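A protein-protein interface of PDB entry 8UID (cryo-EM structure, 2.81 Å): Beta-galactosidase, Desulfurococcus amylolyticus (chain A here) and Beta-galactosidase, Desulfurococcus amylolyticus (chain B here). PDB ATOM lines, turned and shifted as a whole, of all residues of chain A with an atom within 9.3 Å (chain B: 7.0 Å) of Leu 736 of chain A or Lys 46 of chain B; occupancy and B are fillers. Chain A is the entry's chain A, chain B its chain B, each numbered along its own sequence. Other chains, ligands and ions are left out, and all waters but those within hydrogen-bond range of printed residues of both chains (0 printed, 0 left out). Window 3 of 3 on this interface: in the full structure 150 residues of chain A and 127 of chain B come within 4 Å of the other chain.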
ATOM      1  N   ARG A 708      11.003  14.965   8.636  1.00  0.00           N
ATOM      2  CA  ARG A 708      10.443  14.085   7.606  1.00  0.00           C
ATOM      3  C   ARG A 708      10.762  12.656   8.024  1.00  0.00           C
ATOM      4  O   ARG A 708      11.926  12.386   8.289  1.00  0.00           O
ATOM      5  CB  ARG A 708      11.130  14.401   6.268  1.00  0.00           C
ATOM      6  CG  ARG A 708      10.742  15.766   5.691  1.00  0.00           C
ATOM      7  CD  ARG A 708      11.612  16.129   4.476  1.00  0.00           C
ATOM      8  NE  ARG A 708      12.878  16.787   4.864  1.00  0.00           N
ATOM      9  CZ  ARG A 708      14.071  16.649   4.310  1.00  0.00           C
ATOM     10  NH1 ARG A 708      14.327  15.770   3.389  1.00  0.00           N
ATOM     11  NH2 ARG A 708      15.054  17.413   4.678  1.00  0.00           N
ATOM     12  N   PRO A 729      26.683   1.883   8.805  1.00  0.00           N
ATOM     13  CA  PRO A 729      25.256   1.980   8.521  1.00  0.00           C
ATOM     14  C   PRO A 729      24.953   2.196   7.030  1.00  0.00           C
ATOM     15  O   PRO A 729      25.435   3.141   6.413  1.00  0.00           O
ATOM     16  CB  PRO A 729      24.764   3.139   9.387  1.00  0.00           C
ATOM     17  CG  PRO A 729      25.999   4.013   9.549  1.00  0.00           C
ATOM     18  CD  PRO A 729      27.122   2.997   9.628  1.00  0.00           C
ATOM     19  N   GLU A 730      24.070   1.372   6.463  1.00  0.00           N
ATOM     20  CA  GLU A 730      23.545   1.523   5.096  1.00  0.00           C
ATOM     21  C   GLU A 730      22.495   2.634   4.835  1.00  0.00           C
ATOM     22  O   GLU A 730      22.332   2.969   3.660  1.00  0.00           O
ATOM     23  CB  GLU A 730      23.009   0.177   4.575  1.00  0.00           C
ATOM     24  CG  GLU A 730      23.955  -1.028   4.721  1.00  0.00           C
ATOM     25  CD  GLU A 730      25.303  -0.916   3.976  1.00  0.00           C
ATOM     26  OE1 GLU A 730      25.629   0.137   3.389  1.00  0.00           O
ATOM     27  OE2 GLU A 730      26.050  -1.921   3.963  1.00  0.00           O
ATOM     28  N   PRO A 731      21.807   3.298   5.799  1.00  0.00           N
ATOM     29  CA  PRO A 731      20.961   4.455   5.483  1.00  0.00           C
ATOM     30  C   PRO A 731      21.693   5.618   4.808  1.00  0.00           C
ATOM     31  O   PRO A 731      21.026   6.484   4.261  1.00  0.00           O
ATOM     32  CB  PRO A 731      20.330   4.918   6.802  1.00  0.00           C
ATOM     33  CG  PRO A 731      21.337   4.411   7.813  1.00  0.00           C
ATOM     34  CD  PRO A 731      21.656   3.047   7.225  1.00  0.00           C
ATOM     35  N   VAL A 732      23.027   5.641   4.751  1.00  0.00           N
ATOM     36  CA  VAL A 732      23.771   6.591   3.903  1.00  0.00           C
ATOM     37  C   VAL A 732      23.336   6.483   2.434  1.00  0.00           C
ATOM     38  O   VAL A 732      23.144   7.503   1.778  1.00  0.00           O
ATOM     39  CB  VAL A 732      25.291   6.396   4.054  1.00  0.00           C
ATOM     40  CG1 VAL A 732      26.091   7.311   3.123  1.00  0.00           C
ATOM     41  CG2 VAL A 732      25.727   6.697   5.494  1.00  0.00           C
ATOM     42  N   ILE A 733      23.058   5.273   1.935  1.00  0.00           N
ATOM     43  CA  ILE A 733      22.508   5.066   0.584  1.00  0.00           C
ATOM     44  C   ILE A 733      21.124   5.717   0.461  1.00  0.00           C
ATOM     45  O   ILE A 733      20.858   6.427  -0.502  1.00  0.00           O
ATOM     46  CB  ILE A 733      22.458   3.558   0.249  1.00  0.00           C
ATOM     47  CG1 ILE A 733      23.883   2.964   0.178  1.00  0.00           C
ATOM     48  CG2 ILE A 733      21.713   3.311  -1.074  1.00  0.00           C
ATOM     49  CD1 ILE A 733      23.924   1.435   0.234  1.00  0.00           C
ATOM     50  N   LYS A 734      20.238   5.530   1.446  1.00  0.00           N
ATOM     51  CA  LYS A 734      18.877   6.097   1.427  1.00  0.00           C
ATOM     52  C   LYS A 734      18.817   7.596   1.738  1.00  0.00           C
ATOM     53  O   LYS A 734      17.878   8.260   1.314  1.00  0.00           O
ATOM     54  CB  LYS A 734      17.945   5.266   2.323  1.00  0.00           C
ATOM     55  CG  LYS A 734      17.744   3.822   1.818  1.00  0.00           C
ATOM     56  CD  LYS A 734      17.201   3.747   0.380  1.00  0.00           C
ATOM     57  CE  LYS A 734      16.834   2.323  -0.062  1.00  0.00           C
ATOM     58  NZ  LYS A 734      15.550   1.852   0.519  1.00  0.00           N
ATOM     59  N   ALA A 735      19.829   8.159   2.387  1.00  0.00           N
ATOM     60  CA  ALA A 735      20.008   9.599   2.506  1.00  0.00           C
ATOM     61  C   ALA A 735      20.430  10.218   1.161  1.00  0.00           C
ATOM     62  O   ALA A 735      19.901  11.259   0.772  1.00  0.00           O
ATOM     63  CB  ALA A 735      21.020   9.868   3.626  1.00  0.00           C
ATOM     64  N   LEU A 736      21.322   9.559   0.409  1.00  0.00           N
ATOM     65  CA  LEU A 736      21.673   9.955  -0.964  1.00  0.00           C
ATOM     66  C   LEU A 736      20.477   9.800  -1.927  1.00  0.00           C
ATOM     67  O   LEU A 736      20.173  10.712  -2.693  1.00  0.00           O
ATOM     68  CB  LEU A 736      22.881   9.122  -1.440  1.00  0.00           C
ATOM     69  CG  LEU A 736      24.197   9.443  -0.703  1.00  0.00           C
ATOM     70  CD1 LEU A 736      25.201   8.305  -0.884  1.00  0.00           C
ATOM     71  CD2 LEU A 736      24.829  10.725  -1.237  1.00  0.00           C
ATOM     72  N   GLN A 737      19.756   8.680  -1.852  1.00  0.00           N
ATOM     73  CA  GLN A 737      18.548   8.373  -2.634  1.00  0.00           C
ATOM     74  C   GLN A 737      17.268   8.973  -2.007  1.00  0.00           C
ATOM     75  O   GLN A 737      16.257   8.292  -1.841  1.00  0.00           O
ATOM     76  CB  GLN A 737      18.439   6.851  -2.832  1.00  0.00           C
ATOM     77  CG  GLN A 737      19.626   6.249  -3.604  1.00  0.00           C
ATOM     78  CD  GLN A 737      19.552   4.726  -3.720  1.00  0.00           C
ATOM     79  OE1 GLN A 737      18.687   4.052  -3.174  1.00  0.00           O
ATOM     80  NE2 GLN A 737      20.459   4.122  -4.452  1.00  0.00           N
ATOM     81  N   GLU A 738      17.314  10.250  -1.611  1.00  0.00           N
ATOM     82  CA  GLU A 738      16.254  10.961  -0.871  1.00  0.00           C
ATOM     83  C   GLU A 738      15.787  10.202   0.385  1.00  0.00           C
ATOM     84  O   GLU A 738      15.415  10.802   1.399  1.00  0.00           O
ATOM     85  CB  GLU A 738      15.063  11.311  -1.783  1.00  0.00           C
ATOM     86  CG  GLU A 738      15.478  12.132  -3.015  1.00  0.00           C
ATOM     87  CD  GLU A 738      14.280  12.658  -3.821  1.00  0.00           C
ATOM     88  OE1 GLU A 738      13.201  12.023  -3.834  1.00  0.00           O
ATOM     89  OE2 GLU A 738      14.417  13.717  -4.478  1.00  0.00           O
ATOM     90  N   ILE B  12      14.649  12.853   8.929  1.00  0.00           N
ATOM     91  CA  ILE B  12      15.528  13.881   8.364  1.00  0.00           C
ATOM     92  C   ILE B  12      14.963  15.259   8.693  1.00  0.00           C
ATOM     93  O   ILE B  12      13.769  15.485   8.544  1.00  0.00           O
ATOM     94  CB  ILE B  12      15.727  13.685   6.845  1.00  0.00           C
ATOM     95  CG1 ILE B  12      16.157  12.235   6.532  1.00  0.00           C
ATOM     96  CG2 ILE B  12      16.758  14.696   6.313  1.00  0.00           C
ATOM     97  CD1 ILE B  12      16.410  11.931   5.055  1.00  0.00           C
ATOM     98  N   PHE B  43      23.547  11.173  11.593  1.00  0.00           N
ATOM     99  CA  PHE B  43      24.234  11.656  10.404  1.00  0.00           C
ATOM    100  C   PHE B  43      24.062  13.169  10.349  1.00  0.00           C
ATOM    101  O   PHE B  43      22.972  13.673  10.606  1.00  0.00           O
ATOM    102  CB  PHE B  43      23.677  11.005   9.130  1.00  0.00           C
ATOM    103  CG  PHE B  43      23.462   9.507   9.204  1.00  0.00           C
ATOM    104  CD1 PHE B  43      22.365   8.986   9.915  1.00  0.00           C
ATOM    105  CD2 PHE B  43      24.376   8.626   8.607  1.00  0.00           C
ATOM    106  CE1 PHE B  43      22.235   7.605  10.116  1.00  0.00           C
ATOM    107  CE2 PHE B  43      24.248   7.243   8.805  1.00  0.00           C
ATOM    108  CZ  PHE B  43      23.202   6.737   9.591  1.00  0.00           C
ATOM    109  N   VAL B  44      25.117  13.906  10.021  1.00  0.00           N
ATOM    110  CA  VAL B  44      25.051  15.356   9.802  1.00  0.00           C
ATOM    111  C   VAL B  44      25.531  15.619   8.392  1.00  0.00           C
ATOM    112  O   VAL B  44      26.581  15.140   7.971  1.00  0.00           O
ATOM    113  CB  VAL B  44      25.784  16.154  10.887  1.00  0.00           C
ATOM    114  CG1 VAL B  44      25.846  17.650  10.557  1.00  0.00           C
ATOM    115  CG2 VAL B  44      25.046  15.988  12.222  1.00  0.00           C
ATOM    116  N   ASN B  45      24.680  16.294   7.627  1.00  0.00           N
ATOM    117  CA  ASN B  45      24.601  16.156   6.179  1.00  0.00           C
ATOM    118  C   ASN B  45      24.503  14.662   5.812  1.00  0.00           C
ATOM    119  O   ASN B  45      23.875  13.895   6.543  1.00  0.00           O
ATOM    120  CB  ASN B  45      25.691  17.022   5.529  1.00  0.00           C
ATOM    121  CG  ASN B  45      25.407  18.476   5.858  1.00  0.00           C
ATOM    122  OD1 ASN B  45      24.343  18.995   5.562  1.00  0.00           O
ATOM    123  ND2 ASN B  45      26.292  19.162   6.525  1.00  0.00           N
ATOM    124  N   LYS B  46      25.079  14.220   4.694  1.00  0.00           N
ATOM    125  CA  LYS B  46      25.071  12.795   4.311  1.00  0.00           C
ATOM    126  C   LYS B  46      26.151  11.962   5.032  1.00  0.00           C
ATOM    127  O   LYS B  46      26.313  10.784   4.727  1.00  0.00           O
ATOM    128  CB  LYS B  46      25.101  12.678   2.772  1.00  0.00           C
ATOM    129  CG  LYS B  46      23.719  12.381   2.163  1.00  0.00           C
ATOM    130  CD  LYS B  46      22.599  13.403   2.425  1.00  0.00           C
ATOM    131  CE  LYS B  46      22.886  14.768   1.781  1.00  0.00           C
ATOM    132  NZ  LYS B  46      21.647  15.564   1.576  1.00  0.00           N
ATOM    133  N   VAL B  47      26.876  12.543   5.993  1.00  0.00           N
ATOM    134  CA  VAL B  47      28.033  11.928   6.665  1.00  0.00           C
ATOM    135  C   VAL B  47      27.626  11.371   8.029  1.00  0.00           C
ATOM    136  O   VAL B  47      26.999  12.046   8.837  1.00  0.00           O
ATOM    137  CB  VAL B  47      29.196  12.930   6.803  1.00  0.00           C
ATOM    138  CG1 VAL B  47      30.420  12.289   7.461  1.00  0.00           C
ATOM    139  CG2 VAL B  47      29.643  13.469   5.441  1.00  0.00           C
ATOM    140  N   TYR B  48      27.985  10.121   8.302  1.00  0.00           N
ATOM    141  CA  TYR B  48      27.699   9.463   9.569  1.00  0.00           C
ATOM    142  C   TYR B  48      28.583   9.995  10.706  1.00  0.00           C
ATOM    143  O   TYR B  48      29.804   9.869  10.660  1.00  0.00           O
ATOM    144  CB  TYR B  48      27.879   7.956   9.372  1.00  0.00           C
ATOM    145  CG  TYR B  48      27.591   7.122  10.598  1.00  0.00           C
ATOM    146  CD1 TYR B  48      26.429   7.362  11.355  1.00  0.00           C
ATOM    147  CD2 TYR B  48      28.482   6.105  10.979  1.00  0.00           C
ATOM    148  CE1 TYR B  48      26.172   6.606  12.504  1.00  0.00           C
ATOM    149  CE2 TYR B  48      28.203   5.316  12.108  1.00  0.00           C
ATOM    150  CZ  TYR B  48      27.039   5.562  12.859  1.00  0.00           C
ATOM    151  OH  TYR B  48      26.744   4.804  13.933  1.00  0.00           O
ATOM    152  N   TYR B  61      31.038  18.478  10.791  1.00  0.00           N
ATOM    153  CA  TYR B  61      30.207  17.806   9.795  1.00  0.00           C
ATOM    154  C   TYR B  61      29.312  18.764   8.997  1.00  0.00           C
ATOM    155  O   TYR B  61      28.620  18.335   8.071  1.00  0.00           O
ATOM    156  CB  TYR B  61      29.367  16.744  10.508  1.00  0.00           C
ATOM    157  CG  TYR B  61      30.168  15.648  11.184  1.00  0.00           C
ATOM    158  CD1 TYR B  61      30.500  14.491  10.461  1.00  0.00           C
ATOM    159  CD2 TYR B  61      30.555  15.765  12.531  1.00  0.00           C
ATOM    160  CE1 TYR B  61      31.207  13.446  11.079  1.00  0.00           C
ATOM    161  CE2 TYR B  61      31.288  14.733  13.148  1.00  0.00           C
ATOM    162  CZ  TYR B  61      31.611  13.568  12.423  1.00  0.00           C
ATOM    163  OH  TYR B  61      32.294  12.556  13.015  1.00  0.00           O
ATOM    164  N   GLU B  68      21.612  19.393   6.805  1.00  0.00           N
ATOM    165  CA  GLU B  68      20.660  18.369   7.233  1.00  0.00           C
ATOM    166  C   GLU B  68      21.158  17.590   8.452  1.00  0.00           C
ATOM    167  O   GLU B  68      22.351  17.380   8.626  1.00  0.00           O
ATOM    168  CB  GLU B  68      20.329  17.417   6.075  1.00  0.00           C
ATOM    169  CG  GLU B  68      19.376  18.074   5.072  1.00  0.00           C
ATOM    170  CD  GLU B  68      18.877  17.085   4.008  1.00  0.00           C
ATOM    171  OE1 GLU B  68      19.705  16.302   3.486  1.00  0.00           O
ATOM    172  OE2 GLU B  68      17.667  17.111   3.676  1.00  0.00           O
ATOM    173  N   ALA B  70      20.156  13.717   9.920  1.00  0.00           N
ATOM    174  CA  ALA B  70      19.369  12.500   9.842  1.00  0.00           C
ATOM    175  C   ALA B  70      19.570  11.651  11.093  1.00  0.00           C
ATOM    176  O   ALA B  70      20.648  11.625  11.678  1.00  0.00           O
ATOM    177  CB  ALA B  70      19.642  11.749   8.539  1.00  0.00           C
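The backbone carbonyl oxygen (O) of Phe 43 of chain B sits at hydrogen-bond distance from the backbone NH (N) of Ala 70 of chain B (2.9 Å). The backbone NH (N) of Asn 45 of chain B sits at hydrogen-bond distance from the backbone carbonyl oxygen (O) of Glu 68 of chain B (2.8 Å). The side-chain carboxylate of Glu 68 of chain B is in salt-bridge range of the side-chain amino group of Lys 46 of chain B.
Leu 736 of chain A touches one residue of chain B. Of the printed residues of chain A, Phe 43 of chain B touches Pro 729, Pro 731 and Val 732. Asn 45 of chain B touches none of the printed residues of chain A. Of chain A, only Val 732 (3.8 Å), Ala 735 (3.8 Å) and Leu 736 (3.9 Å) come within 4 Å of Lys 46 of chain B. Printed residues of chain A within 4 Å of Tyr 48 of chain B: Pro 729 (3.5 Å). Tyr 61 of chain B touches none of the printed residues of chain A.
O of Ile 12 of chain B sits at hydrogen-bond distance from N of Arg 708 of chain A (2.8 Å). The guanidinium group (NH2) of Arg 708 of chain A is in salt-bridge range of the side-chain carboxylate (OE2) of Glu 68 of chain B, at 2.8 Å.
Of the 11 printed residues of chain A, 7 touch a printed residue of chain B. Hydrophobic or aromatic side chains of chain A within 4 Å of the printed part of chain B: Pro 729, Pro 731, Val 732, Ala 735 and Leu 736. Hydrophobic or aromatic side chains of chain B within 4 Å of the printed part of chain A: Ile 12, Phe 43 and Tyr 48.
Phe 43 of chain B touches Pro 729 of chain A (CE2 to CG, 3.7 Å). Pro 729 of chain A touches Tyr 48 of chain B. CZ of Phe 43 of chain B touches CG of Pro 731 of chain A (3.5 Å). CG2 of Val 732 of chain A touches CE2 of Phe 43 of chain B, 3.7 Å away. Lys 46 of chain B touches Val 732 of chain A (O to CG1, 3.8 Å). Lys 46 of chain B touches Ala 735 of chain A (CD to O, 3.8 Å). Lys 46 of chain B touches Leu 736 of chain A (CG to CD2, 3.9 Å). O of Glu 738 of chain A touches CD1 of Ile 12 of chain B, at 3.95 Å.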
